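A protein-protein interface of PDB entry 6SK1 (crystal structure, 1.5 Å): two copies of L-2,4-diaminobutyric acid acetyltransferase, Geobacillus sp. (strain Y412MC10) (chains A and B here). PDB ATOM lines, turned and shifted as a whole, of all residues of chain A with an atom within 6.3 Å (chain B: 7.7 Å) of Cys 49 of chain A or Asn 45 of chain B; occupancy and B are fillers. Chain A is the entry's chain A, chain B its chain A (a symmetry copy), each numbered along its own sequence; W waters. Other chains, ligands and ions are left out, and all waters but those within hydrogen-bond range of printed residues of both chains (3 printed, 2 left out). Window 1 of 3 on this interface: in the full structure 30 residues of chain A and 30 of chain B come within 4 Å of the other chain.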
ATOM      1  N   LEU A  44      -4.530  23.994 -24.398  1.00  0.00           N
ATOM      2  CA  LEU A  44      -4.769  22.606 -23.918  1.00  0.00           C
ATOM      3  C   LEU A  44      -3.611  22.218 -22.994  1.00  0.00           C
ATOM      4  O   LEU A  44      -2.443  22.268 -23.384  1.00  0.00           O
ATOM      5  CB  LEU A  44      -4.845  21.644 -25.099  1.00  0.00           C
ATOM      6  CG  LEU A  44      -5.105  20.180 -24.819  1.00  0.00           C
ATOM      7  CD1 LEU A  44      -6.451  19.968 -24.175  1.00  0.00           C
ATOM      8  CD2 LEU A  44      -4.944  19.402 -26.126  1.00  0.00           C
ATOM      9  N   ASN A  45      -3.979  21.698 -21.825  1.00  0.00           N
ATOM     10  CA  ASN A  45      -3.009  21.128 -20.902  1.00  0.00           C
ATOM     11  C   ASN A  45      -2.965  19.620 -21.038  1.00  0.00           C
ATOM     12  O   ASN A  45      -3.682  19.028 -21.826  1.00  0.00           O
ATOM     13  CB  ASN A  45      -3.365  21.613 -19.490  1.00  0.00           C
ATOM     14  CG  ASN A  45      -3.357  23.087 -19.390  1.00  0.00           C
ATOM     15  OD1 ASN A  45      -4.540  23.656 -19.192  1.00  0.00           O
ATOM     16  ND2 ASN A  45      -2.361  23.717 -19.725  1.00  0.00           N
ATOM     17  N   SER A  46      -2.082  19.024 -20.241  1.00  0.00           N
ATOM     18  CA  SER A  46      -1.958  17.573 -20.293  1.00  0.00           C
ATOM     19  C   SER A  46      -3.211  16.909 -19.720  1.00  0.00           C
ATOM     20  O   SER A  46      -3.823  17.406 -18.832  1.00  0.00           O
ATOM     21  CB  SER A  46      -0.726  17.071 -19.571  1.00  0.00           C
ATOM     22  OG  SER A  46      -0.799  17.274 -18.147  1.00  0.00           O
ATOM     23  N   PRO A  47      -3.481  15.654 -20.132  1.00  0.00           N
ATOM     24  CA  PRO A  47      -4.458  14.873 -19.428  1.00  0.00           C
ATOM     25  C   PRO A  47      -4.265  14.788 -17.959  1.00  0.00           C
ATOM     26  O   PRO A  47      -5.217  14.908 -17.153  1.00  0.00           O
ATOM     27  CB  PRO A  47      -4.403  13.484 -20.132  1.00  0.00           C
ATOM     28  CG  PRO A  47      -3.883  13.795 -21.475  1.00  0.00           C
ATOM     29  CD  PRO A  47      -2.934  14.952 -21.306  1.00  0.00           C
ATOM     30  N   TYR A  48      -3.010  14.560 -17.551  1.00  0.00           N
ATOM     31  CA  TYR A  48      -2.663  14.515 -16.137  1.00  0.00           C
ATOM     32  C   TYR A  48      -3.122  15.755 -15.383  1.00  0.00           C
ATOM     33  O   TYR A  48      -3.655  15.638 -14.245  1.00  0.00           O
ATOM     34  CB  TYR A  48      -1.150  14.292 -16.001  1.00  0.00           C
ATOM     35  CG  TYR A  48      -0.592  14.173 -14.598  1.00  0.00           C
ATOM     36  CD1 TYR A  48      -1.034  13.233 -13.728  1.00  0.00           C
ATOM     37  CD2 TYR A  48       0.420  14.997 -14.175  1.00  0.00           C
ATOM     38  CE1 TYR A  48      -0.435  13.096 -12.452  1.00  0.00           C
ATOM     39  CE2 TYR A  48       0.957  14.886 -12.925  1.00  0.00           C
ATOM     40  CZ  TYR A  48       0.514  13.974 -12.130  1.00  0.00           C
ATOM     41  OH  TYR A  48       1.090  13.785 -10.832  1.00  0.00           O
ATOM     42  N   CYS A  49      -2.897  16.939 -15.957  1.00  0.00           N
ATOM     43  CA  CYS A  49      -3.401  18.137 -15.327  1.00  0.00           C
ATOM     44  C   CYS A  49      -4.873  18.052 -15.003  1.00  0.00           C
ATOM     45  O   CYS A  49      -5.309  18.392 -13.891  1.00  0.00           O
ATOM     46  CB  CYS A  49      -3.128  19.282 -16.310  1.00  0.00           C
ATOM     47  SG  CYS A  49      -3.743  20.893 -15.702  1.00  0.00           S
ATOM     48  N   TYR A  50      -5.686  17.649 -15.973  1.00  0.00           N
ATOM     49  CA  TYR A  50      -7.090  17.627 -15.729  1.00  0.00           C
ATOM     50  C   TYR A  50      -7.502  16.566 -14.697  1.00  0.00           C
ATOM     51  O   TYR A  50      -8.451  16.787 -13.950  1.00  0.00           O
ATOM     52  CB  TYR A  50      -7.862  17.458 -17.063  1.00  0.00           C
ATOM     53  CG  TYR A  50      -7.645  18.616 -18.033  1.00  0.00           C
ATOM     54  CD1 TYR A  50      -8.186  19.830 -17.807  1.00  0.00           C
ATOM     55  CD2 TYR A  50      -6.855  18.468 -19.129  1.00  0.00           C
ATOM     56  CE1 TYR A  50      -7.858  20.907 -18.589  1.00  0.00           C
ATOM     57  CE2 TYR A  50      -6.568  19.520 -19.922  1.00  0.00           C
ATOM     58  CZ  TYR A  50      -7.076  20.716 -19.678  1.00  0.00           C
ATOM     59  OH  TYR A  50      -6.762  21.801 -20.492  1.00  0.00           O
ATOM     60  N   MET A  51      -6.766  15.491 -14.610  1.00  0.00           N
ATOM     61  CA  MET A  51      -6.934  14.509 -13.542  1.00  0.00           C
ATOM     62  C   MET A  51      -6.713  15.096 -12.174  1.00  0.00           C
ATOM     63  O   MET A  51      -7.517  14.965 -11.245  1.00  0.00           O
ATOM     64  CB  MET A  51      -6.066  13.289 -13.714  1.00  0.00           C
ATOM     65  CG  MET A  51      -6.380  12.524 -14.952  1.00  0.00           C
ATOM     66  SD  MET A  51      -5.191  11.175 -15.186  1.00  0.00           S
ATOM     67  CE  MET A  51      -5.567  10.732 -16.835  1.00  0.00           C
ATOM     68  N   LEU A  52      -5.636  15.870 -12.056  1.00  0.00           N
ATOM     69  CA  LEU A  52      -5.310  16.527 -10.812  1.00  0.00           C
ATOM     70  C   LEU A  52      -6.342  17.533 -10.413  1.00  0.00           C
ATOM     71  O   LEU A  52      -6.698  17.689  -9.216  1.00  0.00           O
ATOM     72  CB  LEU A  52      -3.951  17.132 -10.888  1.00  0.00           C
ATOM     73  CG  LEU A  52      -2.754  16.226 -10.966  1.00  0.00           C
ATOM     74  CD1 LEU A  52      -1.498  17.051 -11.139  1.00  0.00           C
ATOM     75  CD2 LEU A  52      -2.650  15.283  -9.756  1.00  0.00           C
ATOM     76  N   LEU A  53      -6.884  18.256 -11.376  1.00  0.00           N
ATOM     77  CA  LEU A  53      -7.947  19.193 -11.046  1.00  0.00           C
ATOM     78  C   LEU A  53      -9.112  18.507 -10.442  1.00  0.00           C
ATOM     79  O   LEU A  53      -9.717  19.006  -9.471  1.00  0.00           O
ATOM     80  CB  LEU A  53      -8.395  19.994 -12.319  1.00  0.00           C
ATOM     81  CG  LEU A  53      -7.362  20.925 -12.928  1.00  0.00           C
ATOM     82  CD1 LEU A  53      -7.862  21.596 -14.195  1.00  0.00           C
ATOM     83  CD2 LEU A  53      -6.933  22.006 -11.947  1.00  0.00           C
ATOM     84  N   GLY A  54      -9.455  17.358 -10.952  1.00  0.00           N
ATOM     85  CA  GLY A  54     -10.570  16.598 -10.464  1.00  0.00           C
ATOM     86  C   GLY A  54     -10.343  16.094  -9.090  1.00  0.00           C
ATOM     87  O   GLY A  54     -11.320  15.968  -8.327  1.00  0.00           O
ATOM     88  N   TRP A  89      -9.333  29.995 -15.098  1.00  0.00           N
ATOM     89  CA  TRP A  89      -8.288  29.888 -16.119  1.00  0.00           C
ATOM     90  C   TRP A  89      -8.674  29.146 -17.355  1.00  0.00           C
ATOM     91  O   TRP A  89      -7.957  29.249 -18.340  1.00  0.00           O
ATOM     92  CB  TRP A  89      -7.045  29.489 -15.591  1.00  0.00           C
ATOM     93  CG  TRP A  89      -6.982  28.130 -15.015  1.00  0.00           C
ATOM     94  CD1 TRP A  89      -7.466  27.726 -13.808  1.00  0.00           C
ATOM     95  CD2 TRP A  89      -6.066  27.093 -15.485  1.00  0.00           C
ATOM     96  NE1 TRP A  89      -7.105  26.392 -13.583  1.00  0.00           N
ATOM     97  CE2 TRP A  89      -6.189  25.970 -14.557  1.00  0.00           C
ATOM     98  CE3 TRP A  89      -5.100  26.980 -16.589  1.00  0.00           C
ATOM     99  CZ2 TRP A  89      -5.419  24.790 -14.694  1.00  0.00           C
ATOM    100  CZ3 TRP A  89      -4.400  25.811 -16.693  1.00  0.00           C
ATOM    101  CH2 TRP A  89      -4.504  24.706 -15.736  1.00  0.00           C
ATOM    102  N   GLY B  29       7.443  31.702 -18.294  1.00  0.00           N
ATOM    103  CA  GLY B  29       6.583  30.592 -18.735  1.00  0.00           C
ATOM    104  C   GLY B  29       7.017  29.926 -20.027  1.00  0.00           C
ATOM    105  O   GLY B  29       7.011  28.715 -20.115  1.00  0.00           O
ATOM    106  N   TRP B  33       8.184  26.105 -20.352  1.00  0.00           N
ATOM    107  CA  TRP B  33       7.495  25.275 -21.304  1.00  0.00           C
ATOM    108  C   TRP B  33       8.528  24.581 -22.228  1.00  0.00           C
ATOM    109  O   TRP B  33       8.407  23.426 -22.474  1.00  0.00           O
ATOM    110  CB  TRP B  33       6.476  26.110 -22.063  1.00  0.00           C
ATOM    111  CG  TRP B  33       5.701  25.343 -23.055  1.00  0.00           C
ATOM    112  CD1 TRP B  33       4.561  24.618 -22.804  1.00  0.00           C
ATOM    113  CD2 TRP B  33       6.029  25.161 -24.434  1.00  0.00           C
ATOM    114  NE1 TRP B  33       4.177  24.005 -23.960  1.00  0.00           N
ATOM    115  CE2 TRP B  33       5.045  24.331 -24.982  1.00  0.00           C
ATOM    116  CE3 TRP B  33       7.022  25.696 -25.263  1.00  0.00           C
ATOM    117  CZ2 TRP B  33       5.035  23.972 -26.310  1.00  0.00           C
ATOM    118  CZ3 TRP B  33       7.000  25.342 -26.628  1.00  0.00           C
ATOM    119  CH2 TRP B  33       6.006  24.478 -27.105  1.00  0.00           C
ATOM    120  N   GLU B  34       9.456  25.377 -22.747  1.00  0.00           N
ATOM    121  CA  GLU B  34      10.498  24.810 -23.649  1.00  0.00           C
ATOM    122  C   GLU B  34      11.335  23.831 -22.941  1.00  0.00           C
ATOM    123  O   GLU B  34      11.655  22.769 -23.507  1.00  0.00           O
ATOM    124  CB  GLU B  34      11.320  25.987 -24.207  1.00  0.00           C
ATOM    125  CG  GLU B  34      10.616  26.873 -25.220  1.00  0.00           C
ATOM    126  CD  GLU B  34      11.319  28.093 -25.707  1.00  0.00           C
ATOM    127  OE1 GLU B  34      12.214  28.555 -24.951  1.00  0.00           O
ATOM    128  OE2 GLU B  34      10.820  28.641 -26.733  1.00  0.00           O
ATOM    129  N   ILE B  36      10.383  21.785 -20.478  1.00  0.00           N
ATOM    130  CA  ILE B  36       9.586  20.582 -20.321  1.00  0.00           C
ATOM    131  C   ILE B  36       9.371  19.963 -21.688  1.00  0.00           C
ATOM    132  O   ILE B  36       9.492  18.682 -21.806  1.00  0.00           O
ATOM    133  CB  ILE B  36       8.184  20.934 -19.742  1.00  0.00           C
ATOM    134  CG1 ILE B  36       8.260  21.662 -18.376  1.00  0.00           C
ATOM    135  CG2 ILE B  36       7.325  19.658 -19.619  1.00  0.00           C
ATOM    136  CD1 ILE B  36       9.114  20.896 -17.392  1.00  0.00           C
ATOM    137  N   ARG B  37       9.117  20.764 -22.694  1.00  0.00           N
ATOM    138  CA  ARG B  37       8.939  20.260 -24.098  1.00  0.00           C
ATOM    139  C   ARG B  37      10.163  19.422 -24.499  1.00  0.00           C
ATOM    140  O   ARG B  37      10.068  18.290 -24.999  1.00  0.00           O
ATOM    141  CB  ARG B  37       8.717  21.391 -25.014  1.00  0.00           C
ATOM    142  CG  ARG B  37       8.522  20.928 -26.457  1.00  0.00           C
ATOM    143  CD  ARG B  37       8.860  21.931 -27.536  1.00  0.00           C
ATOM    144  NE  ARG B  37      10.209  22.513 -27.397  1.00  0.00           N
ATOM    145  CZ  ARG B  37      10.596  23.718 -27.837  1.00  0.00           C
ATOM    146  NH1 ARG B  37       9.818  24.553 -28.522  1.00  0.00           N
ATOM    147  NH2 ARG B  37      11.826  24.163 -27.505  1.00  0.00           N
ATOM    148  N   SER B  41       8.531  14.915 -22.236  1.00  0.00           N
ATOM    149  CA  SER B  41       7.459  14.519 -21.340  1.00  0.00           C
ATOM    150  C   SER B  41       6.098  14.484 -22.030  1.00  0.00           C
ATOM    151  O   SER B  41       5.700  15.428 -22.671  1.00  0.00           O
ATOM    152  CB  SER B  41       7.389  15.531 -20.199  1.00  0.00           C
ATOM    153  OG  SER B  41       6.300  15.195 -19.329  1.00  0.00           O
ATOM    154  N   LEU B  42       5.322  13.465 -21.714  1.00  0.00           N
ATOM    155  CA  LEU B  42       3.976  13.359 -22.142  1.00  0.00           C
ATOM    156  C   LEU B  42       3.073  14.277 -21.379  1.00  0.00           C
ATOM    157  O   LEU B  42       1.921  14.411 -21.719  1.00  0.00           O
ATOM    158  CB  LEU B  42       3.483  11.898 -21.984  1.00  0.00           C
ATOM    159  CG  LEU B  42       4.189  10.902 -22.868  1.00  0.00           C
ATOM    160  CD1 LEU B  42       3.710   9.486 -22.637  1.00  0.00           C
ATOM    161  CD2 LEU B  42       4.032  11.180 -24.357  1.00  0.00           C
ATOM    162  N   ASP B  43       3.579  14.863 -20.278  1.00  0.00           N
ATOM    163  CA  ASP B  43       2.719  15.637 -19.347  1.00  0.00           C
ATOM    164  C   ASP B  43       2.929  17.126 -19.546  1.00  0.00           C
ATOM    165  O   ASP B  43       2.678  17.895 -18.667  1.00  0.00           O
ATOM    166  CB  ASP B  43       2.993  15.168 -17.959  1.00  0.00           C
ATOM    167  CG  ASP B  43       2.705  13.688 -17.822  1.00  0.00           C
ATOM    168  OD1 ASP B  43       1.699  13.220 -18.291  1.00  0.00           O
ATOM    169  OD2 ASP B  43       3.516  13.025 -17.162  1.00  0.00           O
ATOM    170  N   LEU B  44       3.370  17.553 -20.704  1.00  0.00           N
ATOM    171  CA  LEU B  44       3.576  18.991 -21.027  1.00  0.00           C
ATOM    172  C   LEU B  44       2.213  19.688 -20.974  1.00  0.00           C
ATOM    173  O   LEU B  44       1.273  19.296 -21.665  1.00  0.00           O
ATOM    174  CB  LEU B  44       4.190  19.139 -22.415  1.00  0.00           C
ATOM    175  CG  LEU B  44       4.498  20.531 -22.922  1.00  0.00           C
ATOM    176  CD1 LEU B  44       5.529  21.218 -22.065  1.00  0.00           C
ATOM    177  CD2 LEU B  44       4.917  20.430 -24.389  1.00  0.00           C
ATOM    178  N   ASN B  45       2.187  20.807 -20.253  1.00  0.00           N
ATOM    179  CA  ASN B  45       1.019  21.676 -20.232  1.00  0.00           C
ATOM    180  C   ASN B  45       1.203  22.838 -21.186  1.00  0.00           C
ATOM    181  O   ASN B  45       2.222  22.974 -21.840  1.00  0.00           O
ATOM    182  CB  ASN B  45       0.775  22.099 -18.778  1.00  0.00           C
ATOM    183  CG  ASN B  45       0.560  20.937 -17.890  1.00  0.00           C
ATOM    184  OD1 ASN B  45       1.515  20.715 -16.994  1.00  0.00           O
ATOM    185  ND2 ASN B  45      -0.310  20.118 -18.156  1.00  0.00           N
ATOM    186  N   SER B  46       0.165  23.669 -21.243  1.00  0.00           N
ATOM    187  CA  SER B  46       0.238  24.822 -22.130  1.00  0.00           C
ATOM    188  C   SER B  46       1.262  25.832 -21.611  1.00  0.00           C
ATOM    189  O   SER B  46       1.445  25.986 -20.447  1.00  0.00           O
ATOM    190  CB  SER B  46      -1.106  25.494 -22.318  1.00  0.00           C
ATOM    191  OG  SER B  46      -1.583  26.123 -21.115  1.00  0.00           O
ATOM    192  N   PRO B  47       1.808  26.671 -22.516  1.00  0.00           N
ATOM    193  CA  PRO B  47       2.543  27.818 -22.064  1.00  0.00           C
ATOM    194  C   PRO B  47       1.837  28.679 -21.082  1.00  0.00           C
ATOM    195  O   PRO B  47       2.407  29.136 -20.065  1.00  0.00           O
ATOM    196  CB  PRO B  47       2.910  28.567 -23.380  1.00  0.00           C
ATOM    197  CG  PRO B  47       2.885  27.507 -24.402  1.00  0.00           C
ATOM    198  CD  PRO B  47       1.813  26.536 -23.982  1.00  0.00           C
ATOM    199  N   TYR B  48       0.555  28.947 -21.362  1.00  0.00           N
ATOM    200  CA  TYR B  48      -0.277  29.727 -20.456  1.00  0.00           C
ATOM    201  C   TYR B  48      -0.273  29.175 -19.038  1.00  0.00           C
ATOM    202  O   TYR B  48      -0.183  29.964 -18.057  1.00  0.00           O
ATOM    203  CB  TYR B  48      -1.698  29.811 -21.031  1.00  0.00           C
ATOM    204  CG  TYR B  48      -2.713  30.622 -20.252  1.00  0.00           C
ATOM    205  CD1 TYR B  48      -2.514  31.930 -19.960  1.00  0.00           C
ATOM    206  CD2 TYR B  48      -3.897  30.059 -19.850  1.00  0.00           C
ATOM    207  CE1 TYR B  48      -3.518  32.680 -19.300  1.00  0.00           C
ATOM    208  CE2 TYR B  48      -4.837  30.780 -19.172  1.00  0.00           C
ATOM    209  CZ  TYR B  48      -4.613  32.025 -18.920  1.00  0.00           C
ATOM    210  OH  TYR B  48      -5.598  32.832 -18.265  1.00  0.00           O
ATOM    211  N   CYS B  49      -0.408  27.855 -18.893  1.00  0.00           N
ATOM    212  CA  CYS B  49      -0.311  27.274 -17.575  1.00  0.00           C
ATOM    213  C   CYS B  49       0.940  27.695 -16.841  1.00  0.00           C
ATOM    214  O   CYS B  49       0.896  28.081 -15.662  1.00  0.00           O
ATOM    215  CB  CYS B  49      -0.336  25.755 -17.776  1.00  0.00           C
ATOM    216  SG  CYS B  49      -0.177  24.834 -16.205  1.00  0.00           S
ATOM    217  N   TYR B  50       2.092  27.584 -17.493  1.00  0.00           N
ATOM    218  CA  TYR B  50       3.301  27.900 -16.810  1.00  0.00           C
ATOM    219  C   TYR B  50       3.428  29.394 -16.473  1.00  0.00           C
ATOM    220  O   TYR B  50       4.004  29.735 -15.445  1.00  0.00           O
ATOM    221  CB  TYR B  50       4.522  27.390 -17.619  1.00  0.00           C
ATOM    222  CG  TYR B  50       4.543  25.873 -17.782  1.00  0.00           C
ATOM    223  CD1 TYR B  50       4.819  25.059 -16.743  1.00  0.00           C
ATOM    224  CD2 TYR B  50       4.231  25.296 -18.973  1.00  0.00           C
ATOM    225  CE1 TYR B  50       4.676  23.701 -16.851  1.00  0.00           C
ATOM    226  CE2 TYR B  50       4.133  23.956 -19.089  1.00  0.00           C
ATOM    227  CZ  TYR B  50       4.375  23.165 -18.058  1.00  0.00           C
ATOM    228  OH  TYR B  50       4.257  21.782 -18.180  1.00  0.00           O
ATOM    229  N   LEU B  53       1.447  29.767 -13.280  1.00  0.00           N
ATOM    230  CA  LEU B  53       2.199  29.301 -12.125  1.00  0.00           C
ATOM    231  C   LEU B  53       3.134  30.336 -11.627  1.00  0.00           C
ATOM    232  O   LEU B  53       3.279  30.532 -10.403  1.00  0.00           O
ATOM    233  CB  LEU B  53       2.985  27.987 -12.470  1.00  0.00           C
ATOM    234  CG  LEU B  53       2.146  26.762 -12.788  1.00  0.00           C
ATOM    235  CD1 LEU B  53       2.993  25.566 -13.182  1.00  0.00           C
ATOM    236  CD2 LEU B  53       1.266  26.366 -11.612  1.00  0.00           C
ATOM    237  N   PHE B  73      13.124  22.810 -13.246  1.00  0.00           N
ATOM    238  CA  PHE B  73      11.853  23.345 -12.752  1.00  0.00           C
ATOM    239  C   PHE B  73      11.127  22.371 -11.867  1.00  0.00           C
ATOM    240  O   PHE B  73      11.109  21.153 -12.139  1.00  0.00           O
ATOM    241  CB  PHE B  73      10.926  23.643 -13.942  1.00  0.00           C
ATOM    242  CG  PHE B  73       9.542  24.202 -13.639  1.00  0.00           C
ATOM    243  CD1 PHE B  73       9.429  25.519 -13.193  1.00  0.00           C
ATOM    244  CD2 PHE B  73       8.447  23.453 -13.848  1.00  0.00           C
ATOM    245  CE1 PHE B  73       8.154  26.068 -12.895  1.00  0.00           C
ATOM    246  CE2 PHE B  73       7.144  24.022 -13.589  1.00  0.00           C
ATOM    247  CZ  PHE B  73       7.087  25.273 -13.119  1.00  0.00           C
ATOM    248  N   SER B  75       7.189  22.247  -9.854  1.00  0.00           N
ATOM    249  CA  SER B  75       5.918  22.895  -9.571  1.00  0.00           C
ATOM    250  C   SER B  75       5.173  22.064  -8.550  1.00  0.00           C
ATOM    251  O   SER B  75       5.090  20.833  -8.601  1.00  0.00           O
ATOM    252  CB  SER B  75       5.082  23.162 -10.758  1.00  0.00           C
ATOM    253  OG  SER B  75       4.779  21.934 -11.400  1.00  0.00           O
ATOM    254  N   PHE B  77       1.705  22.567  -5.461  1.00  0.00           N
ATOM    255  CA  PHE B  77       0.642  23.377  -4.836  1.00  0.00           C
ATOM    256  C   PHE B  77       0.350  22.802  -3.465  1.00  0.00           C
ATOM    257  O   PHE B  77       0.467  21.594  -3.219  1.00  0.00           O
ATOM    258  CB  PHE B  77      -0.652  23.392  -5.709  1.00  0.00           C
ATOM    259  CG  PHE B  77      -1.213  22.078  -6.057  1.00  0.00           C
ATOM    260  CD1 PHE B  77      -2.079  21.418  -5.180  1.00  0.00           C
ATOM    261  CD2 PHE B  77      -0.867  21.423  -7.220  1.00  0.00           C
ATOM    262  CE1 PHE B  77      -2.616  20.183  -5.524  1.00  0.00           C
ATOM    263  CE2 PHE B  77      -1.436  20.208  -7.547  1.00  0.00           C
ATOM    264  CZ  PHE B  77      -2.285  19.578  -6.660  1.00  0.00           C
ATOM    265  N   TRP B  89       3.710  18.311  -8.668  1.00  0.00           N
ATOM    266  CA  TRP B  89       3.130  17.712  -9.873  1.00  0.00           C
ATOM    267  C   TRP B  89       4.025  17.684 -11.068  1.00  0.00           C
ATOM    268  O   TRP B  89       3.711  16.971 -12.009  1.00  0.00           O
ATOM    269  CB  TRP B  89       1.835  18.190 -10.154  1.00  0.00           C
ATOM    270  CG  TRP B  89       1.724  19.622 -10.498  1.00  0.00           C
ATOM    271  CD1 TRP B  89       1.776  20.679  -9.642  1.00  0.00           C
ATOM    272  CD2 TRP B  89       1.170  20.111 -11.760  1.00  0.00           C
ATOM    273  NE1 TRP B  89       1.515  21.862 -10.345  1.00  0.00           N
ATOM    274  CE2 TRP B  89       1.074  21.565 -11.642  1.00  0.00           C
ATOM    275  CE3 TRP B  89       0.695  19.481 -13.001  1.00  0.00           C
ATOM    276  CZ2 TRP B  89       0.550  22.373 -12.679  1.00  0.00           C
ATOM    277  CZ3 TRP B  89       0.222  20.306 -13.982  1.00  0.00           C
ATOM    278  CH2 TRP B  89       0.096  21.759 -13.840  1.00  0.00           C
ATOM    279  N   GLN B  90       5.098  18.477 -11.080  1.00  0.00           N
ATOM    280  CA  GLN B  90       6.052  18.372 -12.171  1.00  0.00           C
ATOM    281  C   GLN B  90       7.435  18.638 -11.678  1.00  0.00           C
ATOM    282  O   GLN B  90       7.663  19.577 -10.887  1.00  0.00           O
ATOM    283  CB  GLN B  90       5.728  19.342 -13.292  1.00  0.00           C
ATOM    284  CG  GLN B  90       6.363  19.066 -14.657  1.00  0.00           C
ATOM    285  CD  GLN B  90       5.351  19.440 -15.885  1.00  0.00           C
ATOM    286  OE1 GLN B  90       4.588  20.500 -15.926  1.00  0.00           O
ATOM    287  NE2 GLN B  90       5.249  18.481 -16.858  1.00  0.00           N
ATOM    288  N   PHE B 159      -5.960   7.340 -19.076  1.00  0.00           N
ATOM    289  CA  PHE B 159      -5.434   8.316 -20.021  1.00  0.00           C
ATOM    290  C   PHE B 159      -6.104   8.165 -21.405  1.00  0.00           C
ATOM    291  O   PHE B 159      -6.733   7.118 -21.631  1.00  0.00           O
ATOM    292  CB  PHE B 159      -3.900   8.202 -20.132  1.00  0.00           C
ATOM    293  CG  PHE B 159      -3.208   8.681 -18.891  1.00  0.00           C
ATOM    294  CD1 PHE B 159      -3.051   7.907 -17.784  1.00  0.00           C
ATOM    295  CD2 PHE B 159      -2.738   9.998 -18.808  1.00  0.00           C
ATOM    296  CE1 PHE B 159      -2.454   8.433 -16.645  1.00  0.00           C
ATOM    297  CE2 PHE B 159      -2.190  10.498 -17.663  1.00  0.00           C
ATOM    298  CZ  PHE B 159      -2.074   9.733 -16.559  1.00  0.00           C
HETATM  299  O   HOH W   1      -4.852  26.427 -20.110  1.00  0.00           O
HETATM  300  O   HOH W   2       1.818  17.958 -16.032  1.00  0.00           O
HETATM  301  O   HOH W   3      -0.814  13.468 -19.287  1.00  0.00           O
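ND2 of Asn 45 of chain A lies within hydrogen-bond range of OG of Ser 46 of chain B.
The side-chain hydroxyl of Ser 46 of chain A sits at hydrogen-bond distance from the side-chain amide nitrogen of Asn 45 of chain B.
The backbone carbonyl oxygen of Asp 43 of chain B lies close to the side-chain amide oxygen of Asn 45 of chain B (3.5 Å).
The backbone carbonyl oxygen (O) of Asn 45 of chain B sits close to the indole nitrogen (NE1) of Trp 33 of chain B, at 3.1 Å.
The side-chain hydroxyl (OG) of Ser 46 of chain A lies within hydrogen-bond range of the backbone NH (N) of Cys 49 of chain A, 3.1 Å away.
The side-chain hydroxyl (OG) of Ser 46 of chain B lies within hydrogen-bond range of the backbone NH (N) of Cys 49 of chain B (3.1 Å).
N of Asp 43 of chain B lies within hydrogen-bond range of OG of Ser 41 of chain B (2.9 Å).
The backbone carbonyl oxygen (O) of Ser 75 of chain B lies within hydrogen-bond range of the backbone NH (N) of Trp 89 of chain B (2.9 Å).
Among the printed residues, pairs that only touch across the chains: Cys 49 of chain A with Asn 45 of chain B (3.5 Å), Asn 45 of chain A with Cys 49 of chain B (3.5 Å), Met 51 of chain A with Phe 159 of chain B (3.5 Å), Ser 46 of chain A with Asp 43 of chain B (3.6 Å), Trp 89 of chain A with Tyr 48 of chain B (3.6 Å), Tyr 48 of chain A with Trp 89 of chain B (3.6 Å), Leu 44 of chain A with Ser 46 of chain B (3.7 Å), Ser 46 of chain A with Leu 44 of chain B (3.7 Å), Asn 45 of chain A with Asn 45 of chain B (3.7 Å), Leu 52 of chain A with Trp 89 of chain B (3.7 Å) and Tyr 48 of chain A with Asp 43 of chain B (3.8 Å).
Of the printed residues of chain B, Asn 45 of chain A touches Asn 45 (3.7 Å), Ser 46 (2.9 Å) and Cys 49 (3.5 Å).
Of the printed residues of chain A, Asp 43 of chain B touches Ser 46 and Tyr 48.
Of chain A, only Asn 45, Ser 46 and Cys 49 come within 4 Å of Asn 45 of chain B.
Of the printed residues of chain A, Ser 46 of chain B touches Leu 44 (3.7 Å) and Asn 45 (2.9 Å).
The nearest residue of chain B that does not touch Cys 49 of chain A is Trp 89 of chain B (4.2 Å).
Of the 22 printed residues of chain B, 8 touch a printed residue of chain A.
Hydrophobic or aromatic side chains of chain B that line the printed part of chain A: Tyr 48, Trp 89 and Phe 159.
Among the printed residues, no Asp or Glu carboxylate lies within 4 Å of a Lys or Arg side-chain nitrogen of the other chain.
Leu 44 of chain A touches Ser 46 of chain B, and with the chains exchanged Ser 46 of chain A touches Leu 44 of chain B.
Asn 45 of chain A touches Ser 46 of chain B, and with the chains exchanged Ser 46 of chain A touches Asn 45 of chain B.
Asn 45 of chain A touches Cys 49 of chain B, and with the chains exchanged Cys 49 of chain A touches Asn 45 of chain B.
Tyr 48 of chain A touches Trp 89 of chain B, and with the chains exchanged Trp 89 of chain A touches Tyr 48 of chain B.
9 positions are printed for both chains.
Water W3 lies within hydrogen-bond range of the side-chain carboxylate (OD1) of Asp 43 of chain B (2.7 Å) and the backbone NH (N) of Tyr 48 of chain A (3.0 Å).
Water W2 lies within hydrogen-bond range of O of Asp 43 of chain B (2.8 Å), OD1 of Asn 45 of chain B (2.9 Å) and OG of Ser 46 of chain A (3.4 Å).
Water W1 lies within hydrogen-bond range of OD1 of Asn 45 of chain A (2.9 Å) and OG of Ser 46 of chain B (3.4 Å).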
